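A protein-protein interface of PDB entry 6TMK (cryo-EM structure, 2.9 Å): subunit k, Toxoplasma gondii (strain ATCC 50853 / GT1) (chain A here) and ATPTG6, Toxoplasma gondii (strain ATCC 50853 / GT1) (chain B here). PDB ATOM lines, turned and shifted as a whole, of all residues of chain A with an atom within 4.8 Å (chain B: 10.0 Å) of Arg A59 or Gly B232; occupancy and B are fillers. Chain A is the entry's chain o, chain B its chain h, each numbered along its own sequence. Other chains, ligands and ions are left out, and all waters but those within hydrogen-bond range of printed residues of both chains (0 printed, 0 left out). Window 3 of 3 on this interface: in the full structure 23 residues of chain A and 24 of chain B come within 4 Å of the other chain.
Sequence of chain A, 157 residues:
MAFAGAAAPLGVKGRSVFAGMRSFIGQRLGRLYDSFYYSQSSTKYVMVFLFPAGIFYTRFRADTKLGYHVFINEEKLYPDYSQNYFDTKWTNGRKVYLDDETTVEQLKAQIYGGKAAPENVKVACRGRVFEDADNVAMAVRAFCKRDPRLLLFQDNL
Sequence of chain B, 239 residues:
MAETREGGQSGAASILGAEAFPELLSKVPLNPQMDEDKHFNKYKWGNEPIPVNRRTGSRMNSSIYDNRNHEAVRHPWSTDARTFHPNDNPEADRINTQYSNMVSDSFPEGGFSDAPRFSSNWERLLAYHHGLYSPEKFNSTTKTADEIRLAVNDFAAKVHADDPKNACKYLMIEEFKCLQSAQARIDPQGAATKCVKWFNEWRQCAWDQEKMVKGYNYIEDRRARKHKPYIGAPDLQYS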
ATOM      1  N   ILE A  55      -8.772 -18.903   4.721  1.00  0.00           N
ATOM      2  CA  ILE A  55      -9.334 -19.528   5.911  1.00  0.00           C
ATOM      3  C   ILE A  55      -8.709 -18.933   7.162  1.00  0.00           C
ATOM      4  O   ILE A  55      -9.401 -18.645   8.145  1.00  0.00           O
ATOM      5  CB  ILE A  55      -9.129 -21.049   5.839  1.00  0.00           C
ATOM      6  CG1 ILE A  55     -10.002 -21.647   4.741  1.00  0.00           C
ATOM      7  CG2 ILE A  55      -9.444 -21.688   7.162  1.00  0.00           C
ATOM      8  CD1 ILE A  55      -9.512 -22.956   4.229  1.00  0.00           C
ATOM      9  N   PHE A  56      -7.392 -18.740   7.144  1.00  0.00           N
ATOM     10  CA  PHE A  56      -6.700 -18.133   8.271  1.00  0.00           C
ATOM     11  C   PHE A  56      -7.231 -16.736   8.548  1.00  0.00           C
ATOM     12  O   PHE A  56      -7.550 -16.397   9.690  1.00  0.00           O
ATOM     13  CB  PHE A  56      -5.203 -18.095   7.983  1.00  0.00           C
ATOM     14  CG  PHE A  56      -4.355 -17.805   9.182  1.00  0.00           C
ATOM     15  CD1 PHE A  56      -3.660 -18.814   9.815  1.00  0.00           C
ATOM     16  CD2 PHE A  56      -4.232 -16.514   9.659  1.00  0.00           C
ATOM     17  CE1 PHE A  56      -2.875 -18.547  10.906  1.00  0.00           C
ATOM     18  CE2 PHE A  56      -3.448 -16.241  10.751  1.00  0.00           C
ATOM     19  CZ  PHE A  56      -2.770 -17.259  11.378  1.00  0.00           C
ATOM     20  N   TYR A  57      -7.331 -15.910   7.507  1.00  0.00           N
ATOM     21  CA  TYR A  57      -7.814 -14.548   7.690  1.00  0.00           C
ATOM     22  C   TYR A  57      -9.222 -14.543   8.264  1.00  0.00           C
ATOM     23  O   TYR A  57      -9.505 -13.846   9.245  1.00  0.00           O
ATOM     24  CB  TYR A  57      -7.771 -13.800   6.361  1.00  0.00           C
ATOM     25  CG  TYR A  57      -8.284 -12.384   6.440  1.00  0.00           C
ATOM     26  CD1 TYR A  57      -7.546 -11.395   7.067  1.00  0.00           C
ATOM     27  CD2 TYR A  57      -9.504 -12.035   5.889  1.00  0.00           C
ATOM     28  CE1 TYR A  57      -8.009 -10.102   7.143  1.00  0.00           C
ATOM     29  CE2 TYR A  57      -9.975 -10.746   5.961  1.00  0.00           C
ATOM     30  CZ  TYR A  57      -9.224  -9.781   6.587  1.00  0.00           C
ATOM     31  OH  TYR A  57      -9.691  -8.490   6.662  1.00  0.00           O
ATOM     32  N   THR A  58     -10.118 -15.333   7.673  1.00  0.00           N
ATOM     33  CA  THR A  58     -11.501 -15.354   8.130  1.00  0.00           C
ATOM     34  C   THR A  58     -11.600 -15.822   9.576  1.00  0.00           C
ATOM     35  O   THR A  58     -12.261 -15.183  10.405  1.00  0.00           O
ATOM     36  CB  THR A  58     -12.326 -16.256   7.216  1.00  0.00           C
ATOM     37  OG1 THR A  58     -12.342 -15.715   5.893  1.00  0.00           O
ATOM     38  CG2 THR A  58     -13.734 -16.376   7.719  1.00  0.00           C
ATOM     39  N   ARG A  59     -10.949 -16.940   9.899  1.00  0.00           N
ATOM     40  CA  ARG A  59     -11.053 -17.488  11.244  1.00  0.00           C
ATOM     41  C   ARG A  59     -10.433 -16.554  12.270  1.00  0.00           C
ATOM     42  O   ARG A  59     -10.994 -16.353  13.350  1.00  0.00           O
ATOM     43  CB  ARG A  59     -10.384 -18.858  11.300  1.00  0.00           C
ATOM     44  CG  ARG A  59     -10.491 -19.554  12.638  1.00  0.00           C
ATOM     45  CD  ARG A  59     -11.915 -19.878  12.972  1.00  0.00           C
ATOM     46  NE  ARG A  59     -12.026 -20.566  14.254  1.00  0.00           N
ATOM     47  CZ  ARG A  59     -12.744 -21.661  14.472  1.00  0.00           C
ATOM     48  NH1 ARG A  59     -12.767 -22.191  15.681  1.00  0.00           N
ATOM     49  NH2 ARG A  59     -13.437 -22.229  13.499  1.00  0.00           N
ATOM     50  N   PHE A  60      -9.272 -15.983  11.958  1.00  0.00           N
ATOM     51  CA  PHE A  60      -8.623 -15.059  12.875  1.00  0.00           C
ATOM     52  C   PHE A  60      -9.497 -13.840  13.125  1.00  0.00           C
ATOM     53  O   PHE A  60      -9.693 -13.424  14.272  1.00  0.00           O
ATOM     54  CB  PHE A  60      -7.269 -14.653  12.300  1.00  0.00           C
ATOM     55  CG  PHE A  60      -6.347 -14.045  13.298  1.00  0.00           C
ATOM     56  CD1 PHE A  60      -5.637 -14.843  14.165  1.00  0.00           C
ATOM     57  CD2 PHE A  60      -6.185 -12.681  13.368  1.00  0.00           C
ATOM     58  CE1 PHE A  60      -4.788 -14.293  15.084  1.00  0.00           C
ATOM     59  CE2 PHE A  60      -5.334 -12.127  14.289  1.00  0.00           C
ATOM     60  CZ  PHE A  60      -4.635 -12.936  15.146  1.00  0.00           C
ATOM     61  N   ARG A  61     -10.036 -13.257  12.055  1.00  0.00           N
ATOM     62  CA  ARG A  61     -10.894 -12.089  12.185  1.00  0.00           C
ATOM     63  C   ARG A  61     -12.116 -12.391  13.038  1.00  0.00           C
ATOM     64  O   ARG A  61     -12.486 -11.596  13.909  1.00  0.00           O
ATOM     65  CB  ARG A  61     -11.299 -11.612  10.797  1.00  0.00           C
ATOM     66  CG  ARG A  61     -12.148 -10.379  10.763  1.00  0.00           C
ATOM     67  CD  ARG A  61     -12.483 -10.034   9.344  1.00  0.00           C
ATOM     68  NE  ARG A  61     -13.301 -11.069   8.729  1.00  0.00           N
ATOM     69  CZ  ARG A  61     -13.881 -10.960   7.541  1.00  0.00           C
ATOM     70  NH1 ARG A  61     -13.733  -9.860   6.824  1.00  0.00           N
ATOM     71  NH2 ARG A  61     -14.605 -11.960   7.072  1.00  0.00           N
ATOM     72  N   ALA A  62     -12.759 -13.531  12.803  1.00  0.00           N
ATOM     73  CA  ALA A  62     -13.953 -13.869  13.567  1.00  0.00           C
ATOM     74  C   ALA A  62     -13.618 -14.131  15.029  1.00  0.00           C
ATOM     75  O   ALA A  62     -14.300 -13.636  15.932  1.00  0.00           O
ATOM     76  CB  ALA A  62     -14.635 -15.084  12.953  1.00  0.00           C
ATOM     77  N   ASP A  63     -12.581 -14.928  15.281  1.00  0.00           N
ATOM     78  CA  ASP A  63     -12.246 -15.339  16.633  1.00  0.00           C
ATOM     79  C   ASP A  63     -11.616 -14.216  17.444  1.00  0.00           C
ATOM     80  O   ASP A  63     -11.563 -14.315  18.673  1.00  0.00           O
ATOM     81  CB  ASP A  63     -11.307 -16.537  16.577  1.00  0.00           C
ATOM     82  CG  ASP A  63     -12.006 -17.808  16.138  1.00  0.00           C
ATOM     83  OD1 ASP A  63     -11.375 -18.884  16.185  1.00  0.00           O
ATOM     84  OD2 ASP A  63     -13.189 -17.734  15.748  1.00  0.00           O
ATOM     85  N   THR A  64     -11.123 -13.166  16.792  1.00  0.00           N
ATOM     86  CA  THR A  64     -10.387 -12.106  17.465  1.00  0.00           C
ATOM     87  C   THR A  64     -11.155 -10.793  17.456  1.00  0.00           C
ATOM     88  O   THR A  64     -11.392 -10.209  18.516  1.00  0.00           O
ATOM     89  CB  THR A  64      -9.013 -11.921  16.808  1.00  0.00           C
ATOM     90  OG1 THR A  64      -8.264 -13.138  16.902  1.00  0.00           O
ATOM     91  CG2 THR A  64      -8.248 -10.809  17.471  1.00  0.00           C
ATOM     92  N   ARG B 223     -11.898 -17.197  30.799  1.00  0.00           N
ATOM     93  CA  ARG B 223     -12.743 -17.899  29.854  1.00  0.00           C
ATOM     94  C   ARG B 223     -12.933 -19.344  30.288  1.00  0.00           C
ATOM     95  O   ARG B 223     -12.017 -19.976  30.820  1.00  0.00           O
ATOM     96  CB  ARG B 223     -12.132 -17.818  28.464  1.00  0.00           C
ATOM     97  CG  ARG B 223     -13.113 -18.031  27.360  1.00  0.00           C
ATOM     98  CD  ARG B 223     -12.494 -17.745  26.018  1.00  0.00           C
ATOM     99  NE  ARG B 223     -13.106 -18.529  24.958  1.00  0.00           N
ATOM    100  CZ  ARG B 223     -13.168 -18.138  23.691  1.00  0.00           C
ATOM    101  NH1 ARG B 223     -12.655 -16.972  23.323  1.00  0.00           N
ATOM    102  NH2 ARG B 223     -13.751 -18.912  22.794  1.00  0.00           N
ATOM    103  N   LYS B 228     -16.452 -22.708  23.838  1.00  0.00           N
ATOM    104  CA  LYS B 228     -16.889 -23.214  22.552  1.00  0.00           C
ATOM    105  C   LYS B 228     -17.442 -24.620  22.734  1.00  0.00           C
ATOM    106  O   LYS B 228     -16.800 -25.446  23.390  1.00  0.00           O
ATOM    107  CB  LYS B 228     -15.738 -23.256  21.572  1.00  0.00           C
ATOM    108  CG  LYS B 228     -15.244 -21.919  21.124  1.00  0.00           C
ATOM    109  CD  LYS B 228     -14.576 -22.047  19.782  1.00  0.00           C
ATOM    110  CE  LYS B 228     -13.349 -22.905  19.883  1.00  0.00           C
ATOM    111  NZ  LYS B 228     -12.551 -22.897  18.642  1.00  0.00           N
ATOM    112  N   PRO B 229     -18.606 -24.943  22.168  1.00  0.00           N
ATOM    113  CA  PRO B 229     -19.078 -26.329  22.255  1.00  0.00           C
ATOM    114  C   PRO B 229     -18.269 -27.275  21.399  1.00  0.00           C
ATOM    115  O   PRO B 229     -18.097 -28.442  21.767  1.00  0.00           O
ATOM    116  CB  PRO B 229     -20.535 -26.238  21.780  1.00  0.00           C
ATOM    117  CG  PRO B 229     -20.834 -24.790  21.652  1.00  0.00           C
ATOM    118  CD  PRO B 229     -19.552 -24.104  21.425  1.00  0.00           C
ATOM    119  N   TYR B 230     -17.760 -26.797  20.271  1.00  0.00           N
ATOM    120  CA  TYR B 230     -17.006 -27.602  19.330  1.00  0.00           C
ATOM    121  C   TYR B 230     -15.805 -26.802  18.859  1.00  0.00           C
ATOM    122  O   TYR B 230     -15.884 -25.582  18.701  1.00  0.00           O
ATOM    123  CB  TYR B 230     -17.890 -28.023  18.153  1.00  0.00           C
ATOM    124  CG  TYR B 230     -17.190 -28.836  17.102  1.00  0.00           C
ATOM    125  CD1 TYR B 230     -16.637 -30.064  17.404  1.00  0.00           C
ATOM    126  CD2 TYR B 230     -17.096 -28.380  15.803  1.00  0.00           C
ATOM    127  CE1 TYR B 230     -16.000 -30.807  16.444  1.00  0.00           C
ATOM    128  CE2 TYR B 230     -16.460 -29.112  14.840  1.00  0.00           C
ATOM    129  CZ  TYR B 230     -15.915 -30.328  15.163  1.00  0.00           C
ATOM    130  OH  TYR B 230     -15.278 -31.066  14.196  1.00  0.00           O
ATOM    131  N   ILE B 231     -14.690 -27.497  18.646  1.00  0.00           N
ATOM    132  CA  ILE B 231     -13.441 -26.820  18.313  1.00  0.00           C
ATOM    133  C   ILE B 231     -13.560 -26.085  16.985  1.00  0.00           C
ATOM    134  O   ILE B 231     -13.046 -24.972  16.828  1.00  0.00           O
ATOM    135  CB  ILE B 231     -12.283 -27.831  18.298  1.00  0.00           C
ATOM    136  CG1 ILE B 231     -10.956 -27.110  18.123  1.00  0.00           C
ATOM    137  CG2 ILE B 231     -12.475 -28.854  17.206  1.00  0.00           C
ATOM    138  CD1 ILE B 231      -9.783 -27.950  18.471  1.00  0.00           C
ATOM    139  N   GLY B 232     -14.237 -26.685  16.017  1.00  0.00           N
ATOM    140  CA  GLY B 232     -14.424 -26.058  14.732  1.00  0.00           C
ATOM    141  C   GLY B 232     -15.465 -24.974  14.705  1.00  0.00           C
ATOM    142  O   GLY B 232     -15.688 -24.362  13.657  1.00  0.00           O
ATOM    143  N   ALA B 233     -16.108 -24.719  15.822  1.00  0.00           N
ATOM    144  CA  ALA B 233     -17.093 -23.662  15.883  1.00  0.00           C
ATOM    145  C   ALA B 233     -16.404 -22.314  16.068  1.00  0.00           C
ATOM    146  O   ALA B 233     -15.358 -22.226  16.716  1.00  0.00           O
ATOM    147  CB  ALA B 233     -18.060 -23.903  17.030  1.00  0.00           C
ATOM    148  N   PRO B 234     -16.972 -21.247  15.520  1.00  0.00           N
ATOM    149  CA  PRO B 234     -16.409 -19.918  15.759  1.00  0.00           C
ATOM    150  C   PRO B 234     -16.892 -19.339  17.075  1.00  0.00           C
ATOM    151  O   PRO B 234     -18.062 -19.463  17.443  1.00  0.00           O
ATOM    152  CB  PRO B 234     -16.924 -19.108  14.568  1.00  0.00           C
ATOM    153  CG  PRO B 234     -18.248 -19.717  14.284  1.00  0.00           C
ATOM    154  CD  PRO B 234     -18.115 -21.190  14.592  1.00  0.00           C
ATOM    155  N   ASP B 235     -15.969 -18.702  17.788  1.00  0.00           N
ATOM    156  CA  ASP B 235     -16.276 -18.024  19.042  1.00  0.00           C
ATOM    157  C   ASP B 235     -16.425 -16.543  18.726  1.00  0.00           C
ATOM    158  O   ASP B 235     -15.467 -15.773  18.784  1.00  0.00           O
ATOM    159  CB  ASP B 235     -15.194 -18.284  20.083  1.00  0.00           C
ATOM    160  CG  ASP B 235     -13.806 -18.017  19.556  1.00  0.00           C
ATOM    161  OD1 ASP B 235     -13.682 -17.756  18.346  1.00  0.00           O
ATOM    162  OD2 ASP B 235     -12.843 -18.074  20.348  1.00  0.00           O
ATOM    163  N   LEU B 236     -17.643 -16.155  18.373  1.00  0.00           N
ATOM    164  CA  LEU B 236     -17.928 -14.770  18.040  1.00  0.00           C
ATOM    165  C   LEU B 236     -17.734 -13.889  19.260  1.00  0.00           C
ATOM    166  O   LEU B 236     -18.319 -14.135  20.317  1.00  0.00           O
ATOM    167  CB  LEU B 236     -19.348 -14.635  17.507  1.00  0.00           C
ATOM    168  CG  LEU B 236     -19.690 -15.414  16.240  1.00  0.00           C
ATOM    169  CD1 LEU B 236     -20.982 -14.881  15.680  1.00  0.00           C
ATOM    170  CD2 LEU B 236     -18.581 -15.334  15.206  1.00  0.00           C
ATOM    171  N   GLN B 237     -16.896 -12.872  19.110  1.00  0.00           N
ATOM    172  CA  GLN B 237     -16.516 -12.029  20.227  1.00  0.00           C
ATOM    173  C   GLN B 237     -17.602 -11.003  20.509  1.00  0.00           C
ATOM    174  O   GLN B 237     -18.112 -10.351  19.594  1.00  0.00           O
ATOM    175  CB  GLN B 237     -15.194 -11.327  19.934  1.00  0.00           C
ATOM    176  CG  GLN B 237     -14.030 -12.266  19.765  1.00  0.00           C
ATOM    177  CD  GLN B 237     -13.621 -12.932  21.053  1.00  0.00           C
ATOM    178  OE1 GLN B 237     -13.096 -12.289  21.961  1.00  0.00           O
ATOM    179  NE2 GLN B 237     -13.849 -14.233  21.140  1.00  0.00           N
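NH1 of Arg A59 lies within hydrogen-bond range of O of Ile B231 (3.0 Å). The backbone carbonyl oxygen (O) of Gly B232 is in hydrogen-bond range of the guanidinium group (NH2) of Arg A59 (3.1 Å). The backbone carbonyl oxygen (O) of Ala B233 lies within hydrogen-bond range of the guanidinium group (NH1) of Arg A59. The side-chain carboxylate of Asp B235 sits close to the side-chain carboxylate of Asp A63 (2.6 Å). The side-chain amide nitrogen (NE2) of Gln B237 lies within hydrogen-bond range of the backbone carbonyl oxygen (O) of Asp A63. The guanidinium group of Arg A59 sits close to the side-chain amino group of Lys B228 (3.1 Å).
The side-chain carboxylate (OD2) of Asp B235 lies within salt-bridge range of the guanidinium group (NH2) of Arg B223 (2.7 Å). NZ of Lys B228 sits at hydrogen-bond distance from O of Ile B231, at 2.8 Å. The side-chain amino group of Lys B228 sits close to the backbone carbonyl oxygen of Ala B233, 3.5 Å away. The backbone carbonyl oxygen of Asp B235 is in hydrogen-bond range of the side-chain amide nitrogen of Gln B237 (3.2 Å). NE of Arg A59 lies within salt-bridge range of OD1 of Asp A63 (2.6 Å). The backbone carbonyl oxygen (O) of Phe A60 is in hydrogen-bond range of the side-chain hydroxyl (OG1) of Thr A64, 3.0 Å away.
O of Ala A62 touches O of Asp B235 (3.8 Å). Pro B234 touches Asp A63 (CA to OD2, 3.9 Å). Gln B237 touches Thr A64 (CG to O, 3.6 Å).
No residue of chain B comes within 4 Å of Thr A58. Of chain B, only Lys B228, Ile B231, Gly B232 and Ala B233 come within 4 Å of Arg A59. Ala A62 touches just one residue of chain B: Asp B235. Of chain B, only Pro B234, Asp B235 and Gln B237 come within 4 Å of Asp A63. Arg B223 touches none of the printed residues of chain A. Of chain A, only Arg A59 comes within 4 Å of Gly B232. Printed residues of chain A within 4 Å of Ala B233: Arg A59. Printed residues of chain A within 4 Å of Pro B234: Asp A63 (3.9 Å). The nearest residue of chain B that does not touch Arg A59 is Pro B234 (4.2 Å). The nearest printed residue of chain A that does not touch Asp B235 is Arg A59 (5.2 Å).
Of the 11 printed residues of chain B, 7 touch a printed residue of chain A. Among the printed residues, no Asp or Glu carboxylate lies within 4 Å of a Lys or Arg side-chain nitrogen of the other chain.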
